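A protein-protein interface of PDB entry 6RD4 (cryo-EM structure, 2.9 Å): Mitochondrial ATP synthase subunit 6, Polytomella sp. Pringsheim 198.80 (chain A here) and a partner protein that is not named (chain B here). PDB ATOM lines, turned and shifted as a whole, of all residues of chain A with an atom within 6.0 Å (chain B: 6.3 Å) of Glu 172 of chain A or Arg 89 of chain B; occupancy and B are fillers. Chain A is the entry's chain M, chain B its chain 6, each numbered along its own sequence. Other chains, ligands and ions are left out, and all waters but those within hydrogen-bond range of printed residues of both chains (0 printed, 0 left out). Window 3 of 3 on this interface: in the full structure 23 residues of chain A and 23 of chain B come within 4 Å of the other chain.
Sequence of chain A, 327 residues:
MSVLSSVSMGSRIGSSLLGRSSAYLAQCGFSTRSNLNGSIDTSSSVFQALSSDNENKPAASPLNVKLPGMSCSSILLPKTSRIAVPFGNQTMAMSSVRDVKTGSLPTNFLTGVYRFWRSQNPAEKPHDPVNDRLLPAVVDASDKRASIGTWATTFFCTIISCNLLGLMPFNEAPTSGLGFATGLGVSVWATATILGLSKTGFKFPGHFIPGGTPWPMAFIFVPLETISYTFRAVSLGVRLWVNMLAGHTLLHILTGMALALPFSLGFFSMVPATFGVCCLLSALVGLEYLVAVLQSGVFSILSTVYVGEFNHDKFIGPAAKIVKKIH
O of Phe 170 of chain A is in hydrogen-bond range of NE of Arg 89 of chain B, at 2.9 Å.
The side-chain amide oxygen (OD1) of Asn 171 of chain A is in hydrogen-bond range of the indole nitrogen (NE1) of Trp 85 of chain B (2.8 Å).
The side-chain carboxylate of Glu 172 of chain A lies within salt-bridge range of the guanidinium group of Arg 89 of chain B (3.6 Å).
Of the printed residues of chain A, Arg 89 of chain B touches Phe 170 and Glu 172.
Of the printed residues of chain A, Ile 86 of chain B touches Phe 170.
Of the printed residues of chain A, Gln 93 of chain B touches Phe 170 (3.6 Å).
Printed residues of chain A within 4 Å of Trp 85 of chain B: Asn 171 (2.8 Å).
Leu 87 of chain B touches none of the printed residues of chain A.
Gly 92 of chain B touches none of the printed residues of chain A.
The nearest printed residue of chain A that does not touch Arg 89 of chain B is Asn 171 of chain A (4.005 Å).
O of Ala 90 of chain B sits at hydrogen-bond distance from OG of Ser 94 of chain B, 3.4 Å away.
Among the printed residues, merely in contact across the chains: Phe 170 of chain A with Ala 90 of chain B, Phe 170 of chain A with Gln 93 of chain B and Phe 170 of chain A with Ile 86 of chain B.
Printed residues of chain A that touch a printed residue of chain B: Phe 170, Asn 171 and Glu 172.
Hydrophobic or aromatic side chains of chain A that line the printed part of chain B: Phe 170.
Printed residues of chain B that touch a printed residue of chain A: Trp 85, Ile 86, Arg 89, Ala 90 and Gln 93.
Hydrophobic or aromatic side chains of chain B that line the printed part of chain A: Trp 85, Ile 86 and Ala 90.
Among the printed residues, 6 pairs touch across the chains.
Among the printed residues, Asp or Glu carboxylates within 4 Å of a Lys or Arg side-chain nitrogen of the other chain: Glu 172 of chain A with Arg 89 of chain B.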
ATOM      1  N   CYS A 162     -10.347  11.738   6.053  1.00  0.00           N
ATOM      2  CA  CYS A 162     -11.078  10.490   6.017  1.00  0.00           C
ATOM      3  C   CYS A 162     -11.080   9.781   7.356  1.00  0.00           C
ATOM      4  O   CYS A 162     -12.091   9.197   7.727  1.00  0.00           O
ATOM      5  CB  CYS A 162     -10.487   9.575   4.959  1.00  0.00           C
ATOM      6  SG  CYS A 162     -10.892  10.019   3.290  1.00  0.00           S
ATOM      7  N   LEU A 165     -13.515  11.495   9.678  1.00  0.00           N
ATOM      8  CA  LEU A 165     -14.924  11.259   9.401  1.00  0.00           C
ATOM      9  C   LEU A 165     -15.473  10.126  10.229  1.00  0.00           C
ATOM     10  O   LEU A 165     -16.635  10.169  10.616  1.00  0.00           O
ATOM     11  CB  LEU A 165     -15.171  10.938   7.943  1.00  0.00           C
ATOM     12  CG  LEU A 165     -15.256  12.059   6.958  1.00  0.00           C
ATOM     13  CD1 LEU A 165     -15.377  11.452   5.601  1.00  0.00           C
ATOM     14  CD2 LEU A 165     -16.487  12.811   7.306  1.00  0.00           C
ATOM     15  N   GLY A 166     -14.659   9.127  10.539  1.00  0.00           N
ATOM     16  CA  GLY A 166     -15.109   8.017  11.342  1.00  0.00           C
ATOM     17  C   GLY A 166     -15.462   8.374  12.758  1.00  0.00           C
ATOM     18  O   GLY A 166     -16.132   7.584  13.425  1.00  0.00           O
ATOM     19  N   MET A 168     -16.924  11.469  13.417  1.00  0.00           N
ATOM     20  CA  MET A 168     -18.131  12.260  13.375  1.00  0.00           C
ATOM     21  C   MET A 168     -19.332  11.345  13.530  1.00  0.00           C
ATOM     22  O   MET A 168     -19.296  10.200  13.090  1.00  0.00           O
ATOM     23  CB  MET A 168     -18.233  13.022  12.065  1.00  0.00           C
ATOM     24  CG  MET A 168     -17.139  14.014  11.843  1.00  0.00           C
ATOM     25  SD  MET A 168     -16.958  15.148  13.213  1.00  0.00           S
ATOM     26  CE  MET A 168     -15.327  14.730  13.798  1.00  0.00           C
ATOM     27  N   PHE A 170     -22.893   9.628  12.809  1.00  0.00           N
ATOM     28  CA  PHE A 170     -23.565   9.099  11.626  1.00  0.00           C
ATOM     29  C   PHE A 170     -22.624   8.812  10.477  1.00  0.00           C
ATOM     30  O   PHE A 170     -23.084   8.549   9.372  1.00  0.00           O
ATOM     31  CB  PHE A 170     -24.695  10.005  11.130  1.00  0.00           C
ATOM     32  CG  PHE A 170     -25.655  10.404  12.192  1.00  0.00           C
ATOM     33  CD1 PHE A 170     -26.688   9.570  12.551  1.00  0.00           C
ATOM     34  CD2 PHE A 170     -25.534  11.616  12.825  1.00  0.00           C
ATOM     35  CE1 PHE A 170     -27.561   9.933  13.532  1.00  0.00           C
ATOM     36  CE2 PHE A 170     -26.408  11.981  13.802  1.00  0.00           C
ATOM     37  CZ  PHE A 170     -27.424  11.138  14.151  1.00  0.00           C
ATOM     38  N   ASN A 171     -21.321   8.815  10.699  1.00  0.00           N
ATOM     39  CA  ASN A 171     -20.370   8.693   9.613  1.00  0.00           C
ATOM     40  C   ASN A 171     -19.375   7.593   9.906  1.00  0.00           C
ATOM     41  O   ASN A 171     -19.074   7.298  11.060  1.00  0.00           O
ATOM     42  CB  ASN A 171     -19.629   9.979   9.381  1.00  0.00           C
ATOM     43  CG  ASN A 171     -20.393  10.937   8.556  1.00  0.00           C
ATOM     44  OD1 ASN A 171     -20.660  10.685   7.399  1.00  0.00           O
ATOM     45  ND2 ASN A 171     -20.741  12.063   9.131  1.00  0.00           N
ATOM     46  N   GLU A 172     -18.887   6.976   8.841  1.00  0.00           N
ATOM     47  CA  GLU A 172     -17.809   6.019   8.917  1.00  0.00           C
ATOM     48  C   GLU A 172     -16.628   6.566   8.145  1.00  0.00           C
ATOM     49  O   GLU A 172     -16.773   7.421   7.275  1.00  0.00           O
ATOM     50  CB  GLU A 172     -18.220   4.663   8.360  1.00  0.00           C
ATOM     51  CG  GLU A 172     -18.469   4.663   6.885  1.00  0.00           C
ATOM     52  CD  GLU A 172     -19.271   3.472   6.432  1.00  0.00           C
ATOM     53  OE1 GLU A 172     -19.815   2.758   7.298  1.00  0.00           O
ATOM     54  OE2 GLU A 172     -19.370   3.254   5.206  1.00  0.00           O
ATOM     55  N   ALA A 173     -15.470   6.103   8.502  1.00  0.00           N
ATOM     56  CA  ALA A 173     -14.265   6.530   7.835  1.00  0.00           C
ATOM     57  C   ALA A 173     -14.174   5.840   6.487  1.00  0.00           C
ATOM     58  O   ALA A 173     -14.436   4.642   6.401  1.00  0.00           O
ATOM     59  CB  ALA A 173     -13.061   6.190   8.682  1.00  0.00           C
ATOM     60  N   PRO A 174     -13.855   6.559   5.415  1.00  0.00           N
ATOM     61  CA  PRO A 174     -13.638   5.883   4.143  1.00  0.00           C
ATOM     62  C   PRO A 174     -12.412   5.015   4.150  1.00  0.00           C
ATOM     63  O   PRO A 174     -12.383   4.009   3.441  1.00  0.00           O
ATOM     64  CB  PRO A 174     -13.490   7.039   3.164  1.00  0.00           C
ATOM     65  CG  PRO A 174     -14.104   8.133   3.793  1.00  0.00           C
ATOM     66  CD  PRO A 174     -13.890   8.006   5.230  1.00  0.00           C
ATOM     67  N   SER A 176     -11.598   3.070   6.401  1.00  0.00           N
ATOM     68  CA  SER A 176     -11.955   1.805   7.000  1.00  0.00           C
ATOM     69  C   SER A 176     -12.384   0.795   5.962  1.00  0.00           C
ATOM     70  O   SER A 176     -12.772  -0.311   6.321  1.00  0.00           O
ATOM     71  CB  SER A 176     -13.074   2.016   8.003  1.00  0.00           C
ATOM     72  OG  SER A 176     -13.456   0.794   8.570  1.00  0.00           O
ATOM     73  N   HIS A 248     -12.594   0.659  15.331  1.00  0.00           N
ATOM     74  CA  HIS A 248     -14.038   0.773  15.221  1.00  0.00           C
ATOM     75  C   HIS A 248     -14.739  -0.529  15.576  1.00  0.00           C
ATOM     76  O   HIS A 248     -15.872  -0.509  16.053  1.00  0.00           O
ATOM     77  CB  HIS A 248     -14.417   1.200  13.814  1.00  0.00           C
ATOM     78  CG  HIS A 248     -15.853   1.579  13.673  1.00  0.00           C
ATOM     79  ND1 HIS A 248     -16.426   2.601  14.396  1.00  0.00           N
ATOM     80  CD2 HIS A 248     -16.834   1.069  12.895  1.00  0.00           C
ATOM     81  CE1 HIS A 248     -17.701   2.705  14.068  1.00  0.00           C
ATOM     82  NE2 HIS A 248     -17.973   1.787  13.161  1.00  0.00           N
ATOM     83  N   SER B  84     -29.687  16.237   4.724  1.00  0.00           N
ATOM     84  CA  SER B  84     -30.052  15.132   3.853  1.00  0.00           C
ATOM     85  C   SER B  84     -29.066  13.986   3.951  1.00  0.00           C
ATOM     86  O   SER B  84     -29.383  12.870   3.543  1.00  0.00           O
ATOM     87  CB  SER B  84     -30.148  15.605   2.415  1.00  0.00           C
ATOM     88  OG  SER B  84     -30.306  14.509   1.553  1.00  0.00           O
ATOM     89  N   TRP B  85     -27.855  14.243   4.432  1.00  0.00           N
ATOM     90  CA  TRP B  85     -26.888  13.179   4.646  1.00  0.00           C
ATOM     91  C   TRP B  85     -27.055  12.557   6.014  1.00  0.00           C
ATOM     92  O   TRP B  85     -26.934  11.346   6.156  1.00  0.00           O
ATOM     93  CB  TRP B  85     -25.473  13.718   4.485  1.00  0.00           C
ATOM     94  CG  TRP B  85     -24.415  12.732   4.748  1.00  0.00           C
ATOM     95  CD1 TRP B  85     -23.645  12.643   5.848  1.00  0.00           C
ATOM     96  CD2 TRP B  85     -23.994  11.697   3.876  1.00  0.00           C
ATOM     97  NE1 TRP B  85     -22.774  11.606   5.730  1.00  0.00           N
ATOM     98  CE2 TRP B  85     -22.971  11.007   4.519  1.00  0.00           C
ATOM     99  CE3 TRP B  85     -24.389  11.282   2.611  1.00  0.00           C
ATOM    100  CZ2 TRP B  85     -22.341   9.929   3.944  1.00  0.00           C
ATOM    101  CZ3 TRP B  85     -23.765  10.214   2.051  1.00  0.00           C
ATOM    102  CH2 TRP B  85     -22.754   9.552   2.709  1.00  0.00           C
ATOM    103  N   ILE B  86     -27.343  13.364   7.026  1.00  0.00           N
ATOM    104  CA  ILE B  86     -27.467  12.837   8.377  1.00  0.00           C
ATOM    105  C   ILE B  86     -28.743  12.024   8.514  1.00  0.00           C
ATOM    106  O   ILE B  86     -28.765  10.992   9.185  1.00  0.00           O
ATOM    107  CB  ILE B  86     -27.382  13.996   9.384  1.00  0.00           C
ATOM    108  CG1 ILE B  86     -25.924  14.373   9.595  1.00  0.00           C
ATOM    109  CG2 ILE B  86     -28.006  13.660  10.714  1.00  0.00           C
ATOM    110  CD1 ILE B  86     -25.723  15.496  10.542  1.00  0.00           C
ATOM    111  N   LEU B  87     -29.805  12.431   7.830  1.00  0.00           N
ATOM    112  CA  LEU B  87     -31.023  11.635   7.847  1.00  0.00           C
ATOM    113  C   LEU B  87     -30.861  10.355   7.055  1.00  0.00           C
ATOM    114  O   LEU B  87     -31.395   9.324   7.449  1.00  0.00           O
ATOM    115  CB  LEU B  87     -32.191  12.433   7.295  1.00  0.00           C
ATOM    116  CG  LEU B  87     -32.652  13.549   8.215  1.00  0.00           C
ATOM    117  CD1 LEU B  87     -33.690  14.371   7.517  1.00  0.00           C
ATOM    118  CD2 LEU B  87     -33.180  12.981   9.503  1.00  0.00           C
ATOM    119  N   TYR B  88     -30.127  10.392   5.962  1.00  0.00           N
ATOM    120  CA  TYR B  88     -29.943   9.195   5.165  1.00  0.00           C
ATOM    121  C   TYR B  88     -28.990   8.226   5.828  1.00  0.00           C
ATOM    122  O   TYR B  88     -29.154   7.016   5.694  1.00  0.00           O
ATOM    123  CB  TYR B  88     -29.448   9.591   3.783  1.00  0.00           C
ATOM    124  CG  TYR B  88     -28.680   8.546   3.052  1.00  0.00           C
ATOM    125  CD1 TYR B  88     -29.320   7.478   2.465  1.00  0.00           C
ATOM    126  CD2 TYR B  88     -27.311   8.639   2.924  1.00  0.00           C
ATOM    127  CE1 TYR B  88     -28.618   6.526   1.789  1.00  0.00           C
ATOM    128  CE2 TYR B  88     -26.604   7.690   2.255  1.00  0.00           C
ATOM    129  CZ  TYR B  88     -27.259   6.641   1.689  1.00  0.00           C
ATOM    130  OH  TYR B  88     -26.547   5.698   1.013  1.00  0.00           O
ATOM    131  N   ARG B  89     -27.996   8.727   6.544  1.00  0.00           N
ATOM    132  CA  ARG B  89     -27.098   7.839   7.252  1.00  0.00           C
ATOM    133  C   ARG B  89     -27.735   7.279   8.500  1.00  0.00           C
ATOM    134  O   ARG B  89     -27.436   6.150   8.870  1.00  0.00           O
ATOM    135  CB  ARG B  89     -25.822   8.565   7.617  1.00  0.00           C
ATOM    136  CG  ARG B  89     -24.936   8.832   6.469  1.00  0.00           C
ATOM    137  CD  ARG B  89     -24.282   7.610   5.993  1.00  0.00           C
ATOM    138  NE  ARG B  89     -23.618   6.933   7.082  1.00  0.00           N
ATOM    139  CZ  ARG B  89     -22.675   6.025   6.909  1.00  0.00           C
ATOM    140  NH1 ARG B  89     -22.285   5.705   5.692  1.00  0.00           N
ATOM    141  NH2 ARG B  89     -22.128   5.439   7.952  1.00  0.00           N
ATOM    142  N   ALA B  90     -28.603   8.037   9.163  1.00  0.00           N
ATOM    143  CA  ALA B  90     -29.341   7.510  10.301  1.00  0.00           C
ATOM    144  C   ALA B  90     -30.477   6.609   9.881  1.00  0.00           C
ATOM    145  O   ALA B  90     -30.966   5.836  10.700  1.00  0.00           O
ATOM    146  CB  ALA B  90     -29.908   8.636  11.148  1.00  0.00           C
ATOM    147  N   ASP B  91     -30.925   6.718   8.639  1.00  0.00           N
ATOM    148  CA  ASP B  91     -31.936   5.808   8.133  1.00  0.00           C
ATOM    149  C   ASP B  91     -31.367   4.417   7.960  1.00  0.00           C
ATOM    150  O   ASP B  91     -31.936   3.440   8.450  1.00  0.00           O
ATOM    151  CB  ASP B  91     -32.483   6.329   6.815  1.00  0.00           C
ATOM    152  CG  ASP B  91     -33.240   5.285   6.046  1.00  0.00           C
ATOM    153  OD1 ASP B  91     -34.351   4.907   6.473  1.00  0.00           O
ATOM    154  OD2 ASP B  91     -32.722   4.836   5.004  1.00  0.00           O
ATOM    155  N   GLY B  92     -30.229   4.307   7.282  1.00  0.00           N
ATOM    156  CA  GLY B  92     -29.601   3.021   7.072  1.00  0.00           C
ATOM    157  C   GLY B  92     -28.834   2.503   8.257  1.00  0.00           C
ATOM    158  O   GLY B  92     -28.427   1.343   8.250  1.00  0.00           O
ATOM    159  N   GLN B  93     -28.581   3.346   9.248  1.00  0.00           N
ATOM    160  CA  GLN B  93     -28.038   2.873  10.511  1.00  0.00           C
ATOM    161  C   GLN B  93     -29.085   2.184  11.341  1.00  0.00           C
ATOM    162  O   GLN B  93     -28.746   1.341  12.169  1.00  0.00           O
ATOM    163  CB  GLN B  93     -27.488   4.020  11.340  1.00  0.00           C
ATOM    164  CG  GLN B  93     -26.037   4.295  11.198  1.00  0.00           C
ATOM    165  CD  GLN B  93     -25.603   5.349  12.154  1.00  0.00           C
ATOM    166  OE1 GLN B  93     -26.423   5.983  12.796  1.00  0.00           O
ATOM    167  NE2 GLN B  93     -24.308   5.550  12.261  1.00  0.00           N
ATOM    168  N   SER B  94     -30.342   2.544  11.162  1.00  0.00           N
ATOM    169  CA  SER B  94     -31.415   2.002  11.967  1.00  0.00           C
ATOM    170  C   SER B  94     -31.929   0.680  11.449  1.00  0.00           C
ATOM    171  O   SER B  94     -32.806   0.100  12.077  1.00  0.00           O
ATOM    172  CB  SER B  94     -32.555   2.991  12.021  1.00  0.00           C
ATOM    173  OG  SER B  94     -33.102   3.144  10.732  1.00  0.00           O
